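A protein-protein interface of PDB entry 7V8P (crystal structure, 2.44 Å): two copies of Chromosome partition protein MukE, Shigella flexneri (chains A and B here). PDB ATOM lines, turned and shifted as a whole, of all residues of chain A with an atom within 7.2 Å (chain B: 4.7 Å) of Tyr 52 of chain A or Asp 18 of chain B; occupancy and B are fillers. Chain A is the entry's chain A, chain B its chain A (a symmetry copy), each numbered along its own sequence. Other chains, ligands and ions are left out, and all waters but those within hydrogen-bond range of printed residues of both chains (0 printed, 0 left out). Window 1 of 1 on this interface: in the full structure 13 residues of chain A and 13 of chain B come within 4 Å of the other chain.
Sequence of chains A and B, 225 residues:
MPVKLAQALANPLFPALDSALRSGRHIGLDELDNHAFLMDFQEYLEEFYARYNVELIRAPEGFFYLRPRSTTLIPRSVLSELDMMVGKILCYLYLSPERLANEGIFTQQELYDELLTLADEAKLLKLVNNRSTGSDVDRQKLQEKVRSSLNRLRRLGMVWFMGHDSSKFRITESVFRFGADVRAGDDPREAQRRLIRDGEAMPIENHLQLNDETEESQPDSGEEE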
ATOM      1  N   ASP A  18     -20.101 -28.205  -5.477  1.00  0.00           N
ATOM      2  CA  ASP A  18     -20.853 -27.376  -6.414  1.00  0.00           C
ATOM      3  C   ASP A  18     -19.919 -26.616  -7.347  1.00  0.00           C
ATOM      4  O   ASP A  18     -20.167 -26.536  -8.556  1.00  0.00           O
ATOM      5  CB  ASP A  18     -21.753 -26.407  -5.649  1.00  0.00           C
ATOM      6  CG  ASP A  18     -22.472 -25.434  -6.562  1.00  0.00           C
ATOM      7  OD1 ASP A  18     -23.092 -25.886  -7.546  1.00  0.00           O
ATOM      8  OD2 ASP A  18     -22.422 -24.217  -6.291  1.00  0.00           O
ATOM      9  N   ARG A  22     -19.544 -27.068 -11.417  1.00  0.00           N
ATOM     10  CA  ARG A  22     -19.738 -25.954 -12.341  1.00  0.00           C
ATOM     11  C   ARG A  22     -18.520 -25.731 -13.227  1.00  0.00           C
ATOM     12  O   ARG A  22     -18.647 -25.185 -14.328  1.00  0.00           O
ATOM     13  CB  ARG A  22     -20.072 -24.679 -11.565  1.00  0.00           C
ATOM     14  CG  ARG A  22     -21.494 -24.639 -11.040  1.00  0.00           C
ATOM     15  CD  ARG A  22     -21.710 -23.470 -10.096  1.00  0.00           C
ATOM     16  NE  ARG A  22     -22.850 -23.694  -9.213  1.00  0.00           N
ATOM     17  CZ  ARG A  22     -23.826 -22.814  -9.013  1.00  0.00           C
ATOM     18  NH1 ARG A  22     -23.804 -21.646  -9.638  1.00  0.00           N
ATOM     19  NH2 ARG A  22     -24.826 -23.104  -8.191  1.00  0.00           N
ATOM     20  N   GLU A  46     -30.669 -32.478  -9.148  1.00  0.00           N
ATOM     21  CA  GLU A  46     -31.106 -32.363 -10.535  1.00  0.00           C
ATOM     22  C   GLU A  46     -32.015 -31.156 -10.714  1.00  0.00           C
ATOM     23  O   GLU A  46     -31.814 -30.338 -11.618  1.00  0.00           O
ATOM     24  CB  GLU A  46     -31.822 -33.642 -10.971  1.00  0.00           C
ATOM     25  CG  GLU A  46     -30.903 -34.741 -11.470  1.00  0.00           C
ATOM     26  CD  GLU A  46     -31.625 -36.065 -11.629  1.00  0.00           C
ATOM     27  OE1 GLU A  46     -31.542 -36.905 -10.708  1.00  0.00           O
ATOM     28  OE2 GLU A  46     -32.280 -36.263 -12.673  1.00  0.00           O
ATOM     29  N   GLU A  47     -33.023 -31.028  -9.847  1.00  0.00           N
ATOM     30  CA  GLU A  47     -33.929 -29.886  -9.915  1.00  0.00           C
ATOM     31  C   GLU A  47     -33.186 -28.577  -9.689  1.00  0.00           C
ATOM     32  O   GLU A  47     -33.454 -27.576 -10.366  1.00  0.00           O
ATOM     33  CB  GLU A  47     -35.046 -30.045  -8.884  1.00  0.00           C
ATOM     34  CG  GLU A  47     -35.990 -31.201  -9.158  1.00  0.00           C
ATOM     35  CD  GLU A  47     -37.224 -30.769  -9.921  1.00  0.00           C
ATOM     36  OE1 GLU A  47     -38.091 -30.098  -9.320  1.00  0.00           O
ATOM     37  OE2 GLU A  47     -37.328 -31.099 -11.121  1.00  0.00           O
ATOM     38  N   PHE A  48     -32.252 -28.566  -8.736  1.00  0.00           N
ATOM     39  CA  PHE A  48     -31.497 -27.352  -8.443  1.00  0.00           C
ATOM     40  C   PHE A  48     -30.690 -26.902  -9.654  1.00  0.00           C
ATOM     41  O   PHE A  48     -30.799 -25.754 -10.096  1.00  0.00           O
ATOM     42  CB  PHE A  48     -30.582 -27.588  -7.240  1.00  0.00           C
ATOM     43  CG  PHE A  48     -29.617 -26.467  -6.982  1.00  0.00           C
ATOM     44  CD1 PHE A  48     -30.074 -25.207  -6.629  1.00  0.00           C
ATOM     45  CD2 PHE A  48     -28.252 -26.674  -7.089  1.00  0.00           C
ATOM     46  CE1 PHE A  48     -29.185 -24.175  -6.389  1.00  0.00           C
ATOM     47  CE2 PHE A  48     -27.359 -25.646  -6.852  1.00  0.00           C
ATOM     48  CZ  PHE A  48     -27.826 -24.395  -6.501  1.00  0.00           C
ATOM     49  N   TYR A  49     -29.884 -27.805 -10.213  1.00  0.00           N
ATOM     50  CA  TYR A  49     -29.050 -27.452 -11.353  1.00  0.00           C
ATOM     51  C   TYR A  49     -29.856 -27.261 -12.631  1.00  0.00           C
ATOM     52  O   TYR A  49     -29.385 -26.578 -13.546  1.00  0.00           O
ATOM     53  CB  TYR A  49     -27.972 -28.515 -11.559  1.00  0.00           C
ATOM     54  CG  TYR A  49     -26.865 -28.431 -10.535  1.00  0.00           C
ATOM     55  CD1 TYR A  49     -26.068 -27.299 -10.445  1.00  0.00           C
ATOM     56  CD2 TYR A  49     -26.626 -29.475  -9.652  1.00  0.00           C
ATOM     57  CE1 TYR A  49     -25.059 -27.210  -9.510  1.00  0.00           C
ATOM     58  CE2 TYR A  49     -25.618 -29.397  -8.711  1.00  0.00           C
ATOM     59  CZ  TYR A  49     -24.837 -28.261  -8.646  1.00  0.00           C
ATOM     60  OH  TYR A  49     -23.831 -28.176  -7.712  1.00  0.00           O
ATOM     61  N   ALA A  50     -31.057 -27.841 -12.715  1.00  0.00           N
ATOM     62  CA  ALA A  50     -31.913 -27.601 -13.870  1.00  0.00           C
ATOM     63  C   ALA A  50     -32.317 -26.139 -13.984  1.00  0.00           C
ATOM     64  O   ALA A  50     -32.684 -25.691 -15.077  1.00  0.00           O
ATOM     65  CB  ALA A  50     -33.162 -28.481 -13.800  1.00  0.00           C
ATOM     66  N   ARG A  51     -32.261 -25.390 -12.880  1.00  0.00           N
ATOM     67  CA  ARG A  51     -32.585 -23.970 -12.880  1.00  0.00           C
ATOM     68  C   ARG A  51     -31.480 -23.115 -13.485  1.00  0.00           C
ATOM     69  O   ARG A  51     -31.698 -21.918 -13.700  1.00  0.00           O
ATOM     70  CB  ARG A  51     -32.887 -23.506 -11.451  1.00  0.00           C
ATOM     71  CG  ARG A  51     -34.056 -24.252 -10.817  1.00  0.00           C
ATOM     72  CD  ARG A  51     -34.874 -23.373  -9.913  1.00  0.00           C
ATOM     73  NE  ARG A  51     -34.129 -22.936  -8.741  1.00  0.00           N
ATOM     74  CZ  ARG A  51     -33.963 -21.664  -8.409  1.00  0.00           C
ATOM     75  NH1 ARG A  51     -34.480 -20.704  -9.163  1.00  0.00           N
ATOM     76  NH2 ARG A  51     -33.279 -21.357  -7.322  1.00  0.00           N
ATOM     77  N   TYR A  52     -30.309 -23.695 -13.748  1.00  0.00           N
ATOM     78  CA  TYR A  52     -29.240 -23.043 -14.493  1.00  0.00           C
ATOM     79  C   TYR A  52     -29.209 -23.485 -15.949  1.00  0.00           C
ATOM     80  O   TYR A  52     -28.224 -23.219 -16.646  1.00  0.00           O
ATOM     81  CB  TYR A  52     -27.882 -23.326 -13.842  1.00  0.00           C
ATOM     82  CG  TYR A  52     -27.718 -22.743 -12.458  1.00  0.00           C
ATOM     83  CD1 TYR A  52     -28.260 -23.377 -11.348  1.00  0.00           C
ATOM     84  CD2 TYR A  52     -27.020 -21.558 -12.260  1.00  0.00           C
ATOM     85  CE1 TYR A  52     -28.112 -22.849 -10.081  1.00  0.00           C
ATOM     86  CE2 TYR A  52     -26.866 -21.022 -10.995  1.00  0.00           C
ATOM     87  CZ  TYR A  52     -27.416 -21.671  -9.910  1.00  0.00           C
ATOM     88  OH  TYR A  52     -27.270 -21.143  -8.647  1.00  0.00           O
ATOM     89  N   ASN A  53     -30.259 -24.166 -16.412  1.00  0.00           N
ATOM     90  CA  ASN A  53     -30.326 -24.725 -17.763  1.00  0.00           C
ATOM     91  C   ASN A  53     -29.150 -25.652 -18.051  1.00  0.00           C
ATOM     92  O   ASN A  53     -28.674 -25.742 -19.185  1.00  0.00           O
ATOM     93  CB  ASN A  53     -30.420 -23.623 -18.819  1.00  0.00           C
ATOM     94  CG  ASN A  53     -31.592 -22.695 -18.581  1.00  0.00           C
ATOM     95  OD1 ASN A  53     -32.470 -22.987 -17.768  1.00  0.00           O
ATOM     96  ND2 ASN A  53     -31.614 -21.571 -19.286  1.00  0.00           N
ATOM     97  N   VAL A  54     -28.668 -26.337 -17.016  1.00  0.00           N
ATOM     98  CA  VAL A  54     -27.713 -27.424 -17.161  1.00  0.00           C
ATOM     99  C   VAL A  54     -28.351 -28.676 -16.577  1.00  0.00           C
ATOM    100  O   VAL A  54     -29.275 -28.612 -15.761  1.00  0.00           O
ATOM    101  CB  VAL A  54     -26.360 -27.125 -16.479  1.00  0.00           C
ATOM    102  CG1 VAL A  54     -25.840 -25.758 -16.903  1.00  0.00           C
ATOM    103  CG2 VAL A  54     -26.490 -27.210 -14.966  1.00  0.00           C
ATOM    104  N   GLU A  55     -27.856 -29.827 -17.016  1.00  0.00           N
ATOM    105  CA  GLU A  55     -28.394 -31.117 -16.606  1.00  0.00           C
ATOM    106  C   GLU A  55     -27.341 -31.865 -15.803  1.00  0.00           C
ATOM    107  O   GLU A  55     -26.248 -32.140 -16.311  1.00  0.00           O
ATOM    108  CB  GLU A  55     -28.826 -31.944 -17.818  1.00  0.00           C
ATOM    109  CG  GLU A  55     -30.071 -31.428 -18.516  1.00  0.00           C
ATOM    110  CD  GLU A  55     -30.107 -31.804 -19.984  1.00  0.00           C
ATOM    111  OE1 GLU A  55     -29.164 -31.436 -20.717  1.00  0.00           O
ATOM    112  OE2 GLU A  55     -31.077 -32.470 -20.404  1.00  0.00           O
ATOM    113  N   LEU A  66     -22.043 -32.112 -14.875  1.00  0.00           N
ATOM    114  CA  LEU A  66     -23.010 -31.161 -15.405  1.00  0.00           C
ATOM    115  C   LEU A  66     -22.839 -31.062 -16.913  1.00  0.00           C
ATOM    116  O   LEU A  66     -21.725 -30.849 -17.403  1.00  0.00           O
ATOM    117  CB  LEU A  66     -22.836 -29.778 -14.774  1.00  0.00           C
ATOM    118  CG  LEU A  66     -22.771 -29.634 -13.254  1.00  0.00           C
ATOM    119  CD1 LEU A  66     -22.708 -28.158 -12.885  1.00  0.00           C
ATOM    120  CD2 LEU A  66     -23.961 -30.305 -12.593  1.00  0.00           C
ATOM    121  N   PRO A  68     -24.237 -28.760 -19.942  1.00  0.00           N
ATOM    122  CA  PRO A  68     -25.037 -27.551 -20.156  1.00  0.00           C
ATOM    123  C   PRO A  68     -25.887 -27.636 -21.412  1.00  0.00           C
ATOM    124  O   PRO A  68     -25.439 -28.096 -22.465  1.00  0.00           O
ATOM    125  CB  PRO A  68     -23.975 -26.452 -20.281  1.00  0.00           C
ATOM    126  CG  PRO A  68     -22.791 -27.152 -20.851  1.00  0.00           C
ATOM    127  CD  PRO A  68     -22.820 -28.560 -20.298  1.00  0.00           C
ATOM    128  N   ARG A  69     -27.133 -27.192 -21.284  1.00  0.00           N
ATOM    129  CA  ARG A  69     -27.994 -27.005 -22.439  1.00  0.00           C
ATOM    130  C   ARG A  69     -27.597 -25.721 -23.168  1.00  0.00           C
ATOM    131  O   ARG A  69     -26.860 -24.883 -22.642  1.00  0.00           O
ATOM    132  CB  ARG A  69     -29.465 -26.965 -22.005  1.00  0.00           C
ATOM    133  CG  ARG A  69     -30.489 -26.985 -23.136  1.00  0.00           C
ATOM    134  CD  ARG A  69     -30.758 -28.392 -23.644  1.00  0.00           C
ATOM    135  NE  ARG A  69     -31.469 -28.377 -24.920  1.00  0.00           N
ATOM    136  CZ  ARG A  69     -30.874 -28.328 -26.108  1.00  0.00           C
ATOM    137  NH1 ARG A  69     -29.551 -28.293 -26.190  1.00  0.00           N
ATOM    138  NH2 ARG A  69     -31.604 -28.316 -27.215  1.00  0.00           N
ATOM    139  N   THR A  71     -28.991 -23.092 -23.591  1.00  0.00           N
ATOM    140  CA  THR A  71     -29.370 -21.888 -22.862  1.00  0.00           C
ATOM    141  C   THR A  71     -28.796 -21.856 -21.450  1.00  0.00           C
ATOM    142  O   THR A  71     -29.400 -21.256 -20.553  1.00  0.00           O
ATOM    143  CB  THR A  71     -30.891 -21.760 -22.812  1.00  0.00           C
ATOM    144  OG1 THR A  71     -31.460 -23.003 -22.382  1.00  0.00           O
ATOM    145  CG2 THR A  71     -31.439 -21.404 -24.184  1.00  0.00           C
ATOM    146  N   THR A  72     -27.642 -22.487 -21.236  1.00  0.00           N
ATOM    147  CA  THR A  72     -27.046 -22.536 -19.907  1.00  0.00           C
ATOM    148  C   THR A  72     -26.799 -21.132 -19.369  1.00  0.00           C
ATOM    149  O   THR A  72     -26.484 -20.204 -20.120  1.00  0.00           O
ATOM    150  CB  THR A  72     -25.729 -23.312 -19.942  1.00  0.00           C
ATOM    151  OG1 THR A  72     -25.030 -23.132 -18.704  1.00  0.00           O
ATOM    152  CG2 THR A  72     -24.852 -22.825 -21.087  1.00  0.00           C
ATOM    153  N   LEU A  73     -26.964 -20.977 -18.058  1.00  0.00           N
ATOM    154  CA  LEU A  73     -26.610 -19.733 -17.390  1.00  0.00           C
ATOM    155  C   LEU A  73     -25.169 -19.731 -16.902  1.00  0.00           C
ATOM    156  O   LEU A  73     -24.651 -18.669 -16.541  1.00  0.00           O
ATOM    157  CB  LEU A  73     -27.560 -19.467 -16.215  1.00  0.00           C
ATOM    158  CG  LEU A  73     -29.065 -19.635 -16.462  1.00  0.00           C
ATOM    159  CD1 LEU A  73     -29.868 -19.037 -15.316  1.00  0.00           C
ATOM    160  CD2 LEU A  73     -29.489 -19.010 -17.786  1.00  0.00           C
ATOM    161  N   ILE A  74     -24.518 -20.889 -16.887  1.00  0.00           N
ATOM    162  CA  ILE A  74     -23.093 -21.004 -16.593  1.00  0.00           C
ATOM    163  C   ILE A  74     -22.342 -20.961 -17.919  1.00  0.00           C
ATOM    164  O   ILE A  74     -22.642 -21.759 -18.820  1.00  0.00           O
ATOM    165  CB  ILE A  74     -22.780 -22.294 -15.820  1.00  0.00           C
ATOM    166  CG1 ILE A  74     -23.682 -22.414 -14.591  1.00  0.00           C
ATOM    167  CG2 ILE A  74     -21.312 -22.335 -15.422  1.00  0.00           C
ATOM    168  CD1 ILE A  74     -23.564 -23.743 -13.881  1.00  0.00           C
ATOM    169  N   PHE B  14     -32.150 -15.600  -8.978  1.00  0.00           N
ATOM    170  CA  PHE B  14     -30.882 -16.025  -8.388  1.00  0.00           C
ATOM    171  C   PHE B  14     -29.988 -16.802  -9.346  1.00  0.00           C
ATOM    172  O   PHE B  14     -28.810 -16.427  -9.481  1.00  0.00           O
ATOM    173  CB  PHE B  14     -31.140 -16.826  -7.109  1.00  0.00           C
ATOM    174  CG  PHE B  14     -29.888 -17.386  -6.496  1.00  0.00           C
ATOM    175  CD1 PHE B  14     -29.027 -16.569  -5.785  1.00  0.00           C
ATOM    176  CD2 PHE B  14     -29.563 -18.726  -6.646  1.00  0.00           C
ATOM    177  CE1 PHE B  14     -27.870 -17.077  -5.225  1.00  0.00           C
ATOM    178  CE2 PHE B  14     -28.407 -19.239  -6.090  1.00  0.00           C
ATOM    179  CZ  PHE B  14     -27.557 -18.414  -5.379  1.00  0.00           C
ATOM    180  N   PRO B  15     -30.441 -17.872 -10.019  1.00  0.00           N
ATOM    181  CA  PRO B  15     -29.496 -18.647 -10.847  1.00  0.00           C
ATOM    182  C   PRO B  15     -28.786 -17.814 -11.900  1.00  0.00           C
ATOM    183  O   PRO B  15     -27.590 -18.019 -12.141  1.00  0.00           O
ATOM    184  CB  PRO B  15     -30.385 -19.732 -11.477  1.00  0.00           C
ATOM    185  CG  PRO B  15     -31.785 -19.249 -11.312  1.00  0.00           C
ATOM    186  CD  PRO B  15     -31.788 -18.470 -10.041  1.00  0.00           C
ATOM    187  N   ALA B  16     -29.486 -16.868 -12.529  1.00  0.00           N
ATOM    188  CA  ALA B  16     -28.829 -15.989 -13.490  1.00  0.00           C
ATOM    189  C   ALA B  16     -27.869 -15.033 -12.795  1.00  0.00           C
ATOM    190  O   ALA B  16     -26.763 -14.784 -13.290  1.00  0.00           O
ATOM    191  CB  ALA B  16     -29.873 -15.213 -14.292  1.00  0.00           C
ATOM    192  N   LEU B  17     -28.271 -14.491 -11.645  1.00  0.00           N
ATOM    193  CA  LEU B  17     -27.411 -13.553 -10.931  1.00  0.00           C
ATOM    194  C   LEU B  17     -26.269 -14.274 -10.226  1.00  0.00           C
ATOM    195  O   LEU B  17     -25.144 -13.763 -10.175  1.00  0.00           O
ATOM    196  CB  LEU B  17     -28.241 -12.747  -9.935  1.00  0.00           C
ATOM    197  CG  LEU B  17     -27.510 -11.703  -9.095  1.00  0.00           C
ATOM    198  CD1 LEU B  17     -26.783 -10.714  -9.986  1.00  0.00           C
ATOM    199  CD2 LEU B  17     -28.510 -10.991  -8.210  1.00  0.00           C
ATOM    200  N   ASP B  18     -26.540 -15.459  -9.674  1.00  0.00           N
ATOM    201  CA  ASP B  18     -25.483 -16.229  -9.026  1.00  0.00           C
ATOM    202  C   ASP B  18     -24.384 -16.595 -10.014  1.00  0.00           C
ATOM    203  O   ASP B  18     -23.193 -16.492  -9.697  1.00  0.00           O
ATOM    204  CB  ASP B  18     -26.069 -17.487  -8.385  1.00  0.00           C
ATOM    205  CG  ASP B  18     -25.007 -18.393  -7.798  1.00  0.00           C
ATOM    206  OD1 ASP B  18     -24.156 -17.896  -7.032  1.00  0.00           O
ATOM    207  OD2 ASP B  18     -25.025 -19.604  -8.099  1.00  0.00           O
ATOM    208  N   SER B  19     -24.766 -17.017 -11.222  1.00  0.00           N
ATOM    209  CA  SER B  19     -23.775 -17.345 -12.240  1.00  0.00           C
ATOM    210  C   SER B  19     -22.991 -16.107 -12.656  1.00  0.00           C
ATOM    211  O   SER B  19     -21.761 -16.144 -12.767  1.00  0.00           O
ATOM    212  CB  SER B  19     -24.459 -17.981 -13.449  1.00  0.00           C
ATOM    213  OG  SER B  19     -25.522 -18.826 -13.049  1.00  0.00           O
ATOM    214  N   ALA B  20     -23.695 -14.997 -12.897  1.00  0.00           N
ATOM    215  CA  ALA B  20     -23.020 -13.754 -13.260  1.00  0.00           C
ATOM    216  C   ALA B  20     -22.021 -13.339 -12.188  1.00  0.00           C
ATOM    217  O   ALA B  20     -20.891 -12.947 -12.503  1.00  0.00           O
ATOM    218  CB  ALA B  20     -24.049 -12.648 -13.495  1.00  0.00           C
ATOM    219  N   LEU B  21     -22.418 -13.428 -10.916  1.00  0.00           N
ATOM    220  CA  LEU B  21     -21.508 -13.105  -9.822  1.00  0.00           C
ATOM    221  C   LEU B  21     -20.273 -13.999  -9.849  1.00  0.00           C
ATOM    222  O   LEU B  21     -19.141 -13.515  -9.745  1.00  0.00           O
ATOM    223  CB  LEU B  21     -22.236 -13.237  -8.483  1.00  0.00           C
ATOM    224  CG  LEU B  21     -23.166 -12.094  -8.074  1.00  0.00           C
ATOM    225  CD1 LEU B  21     -23.945 -12.458  -6.820  1.00  0.00           C
ATOM    226  CD2 LEU B  21     -22.377 -10.815  -7.859  1.00  0.00           C
ATOM    227  N   ARG B  22     -20.477 -15.312  -9.992  1.00  0.00           N
ATOM    228  CA  ARG B  22     -19.355 -16.247  -9.944  1.00  0.00           C
ATOM    229  C   ARG B  22     -18.400 -16.048 -11.112  1.00  0.00           C
ATOM    230  O   ARG B  22     -17.216 -16.389 -11.009  1.00  0.00           O
ATOM    231  CB  ARG B  22     -19.871 -17.686  -9.917  1.00  0.00           C
ATOM    232  CG  ARG B  22     -20.428 -18.110  -8.572  1.00  0.00           C
ATOM    233  CD  ARG B  22     -21.125 -19.456  -8.653  1.00  0.00           C
ATOM    234  NE  ARG B  22     -22.075 -19.638  -7.560  1.00  0.00           N
ATOM    235  CZ  ARG B  22     -22.128 -20.717  -6.787  1.00  0.00           C
ATOM    236  NH1 ARG B  22     -21.282 -21.717  -6.984  1.00  0.00           N
ATOM    237  NH2 ARG B  22     -23.027 -20.796  -5.814  1.00  0.00           N
ATOM    238  N   PHE B  48     -23.857 -16.935   2.533  1.00  0.00           N
ATOM    239  CA  PHE B  48     -23.873 -18.006   1.542  1.00  0.00           C
ATOM    240  C   PHE B  48     -22.569 -18.046   0.757  1.00  0.00           C
ATOM    241  O   PHE B  48     -21.909 -19.088   0.678  1.00  0.00           O
ATOM    242  CB  PHE B  48     -25.065 -17.823   0.601  1.00  0.00           C
ATOM    243  CG  PHE B  48     -25.058 -18.755  -0.576  1.00  0.00           C
ATOM    244  CD1 PHE B  48     -25.167 -20.125  -0.395  1.00  0.00           C
ATOM    245  CD2 PHE B  48     -24.946 -18.262  -1.865  1.00  0.00           C
ATOM    246  CE1 PHE B  48     -25.163 -20.985  -1.478  1.00  0.00           C
ATOM    247  CE2 PHE B  48     -24.940 -19.115  -2.952  1.00  0.00           C
ATOM    248  CZ  PHE B  48     -25.049 -20.478  -2.758  1.00  0.00           C
ATOM    249  N   TYR B  49     -22.174 -16.910   0.181  1.00  0.00           N
ATOM    250  CA  TYR B  49     -20.956 -16.866  -0.617  1.00  0.00           C
ATOM    251  C   TYR B  49     -19.696 -16.968   0.231  1.00  0.00           C
ATOM    252  O   TYR B  49     -18.647 -17.356  -0.292  1.00  0.00           O
ATOM    253  CB  TYR B  49     -20.931 -15.588  -1.456  1.00  0.00           C
ATOM    254  CG  TYR B  49     -21.876 -15.640  -2.631  1.00  0.00           C
ATOM    255  CD1 TYR B  49     -21.709 -16.586  -3.633  1.00  0.00           C
ATOM    256  CD2 TYR B  49     -22.942 -14.757  -2.733  1.00  0.00           C
ATOM    257  CE1 TYR B  49     -22.570 -16.646  -4.708  1.00  0.00           C
ATOM    258  CE2 TYR B  49     -23.811 -14.809  -3.805  1.00  0.00           C
ATOM    259  CZ  TYR B  49     -23.619 -15.755  -4.790  1.00  0.00           C
ATOM    260  OH  TYR B  49     -24.480 -15.813  -5.861  1.00  0.00           O
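OD2 of Asp 18 of chain A lies within salt-bridge range of NH1 of Arg 22 of chain B (2.8 Å). NE of Arg 22 of chain A lies close to NH1 of Arg 22 of chain B, 3.4 Å away. The side-chain hydroxyl (OH) of Tyr 52 of chain A lies within hydrogen-bond range of the side-chain carboxylate (OD2) of Asp 18 of chain B (2.8 Å). NH1 of Arg 22 of chain A lies within salt-bridge range of OD2 of Asp 18 of chain B (2.8 Å).
The side-chain carboxylate (OD1) of Asp 18 of chain A lies within hydrogen-bond range of the side-chain hydroxyl (OH) of Tyr 49 of chain A (2.4 Å). OD1 of Asp 18 of chain B sits at hydrogen-bond distance from OH of Tyr 49 of chain B, 2.4 Å away. NH2 of Arg 22 of chain A is in hydrogen-bond range of OH of Tyr 52 of chain A (3.2 Å). The side-chain carboxylate (OD1) of Asp 18 of chain A lies within salt-bridge range of the guanidinium group (NE) of Arg 22 of chain A (2.8 Å). O of Tyr 52 of chain A sits at hydrogen-bond distance from N of Leu 73 of chain A, 2.9 Å away. The side-chain carboxylate (OD1) of Asp 18 of chain B is in salt-bridge range of the guanidinium group (NE) of Arg 22 of chain B, at 2.8 Å.
Arg 51 of chain A touches Pro 15 of chain B. Tyr 52 of chain A touches Phe 14 of chain B. CE2 of Tyr 52 of chain A touches O of Pro 15 of chain B, 3.3 Å away. CD2 of Tyr 52 of chain A touches OG of Ser 19 of chain B, at 3.2 Å. Pro 15 of chain B touches Leu 73 of chain A (C to CD1, 3.8 Å). N of Ala 16 of chain B touches CD1 of Leu 73 of chain A, at 3.6 Å. Ser 19 of chain B touches Leu 73 of chain A (CB to O, 3.2 Å).
Printed residues of chain B within 4 Å of Asp 18 of chain A: Arg 22 (2.8 Å). Of the printed residues of chain B, Arg 22 of chain A touches Asp 18 (2.8 Å) and Arg 22 (3.4 Å). Tyr 52 of chain A touches just these residues of chain B: Phe 14, Pro 15, Asp 18 and Ser 19. Of the printed residues of chain A, Ala 16 of chain B touches Leu 73. Of chain A, only Arg 22 (2.8 Å) and Tyr 52 (2.8 Å) come within 4 Å of Asp 18 of chain B. The nearest printed residue of chain B that does not touch Tyr 52 of chain A is Arg 22 of chain B (5.1 Å). The nearest residue of chain A that does not touch Asp 18 of chain B is Asp 18 of chain A (5.6 Å).
Printed residues of chain B that touch a printed residue of chain A: Phe 14, Pro 15, Ala 16, Asp 18, Ser 19 and Arg 22. Among the printed residues, Asp or Glu carboxylates within 4 Å of a Lys or Arg side-chain nitrogen of the other chain: Asp 18 of chain A with Arg 22 of chain B and Arg 22 of chain A with Asp 18 of chain B.
Asp 18 of chain A touches Arg 22 of chain B, and with the chains exchanged Arg 22 of chain A touches Asp 18 of chain B. Arg 22 of chain B touches its own counterpart, Arg 22 of chain A. 4 positions are printed for both chains. Of the 11 pairs that touch across the chains among the printed residues, 3 have their exchanged pair printed and touching as well.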
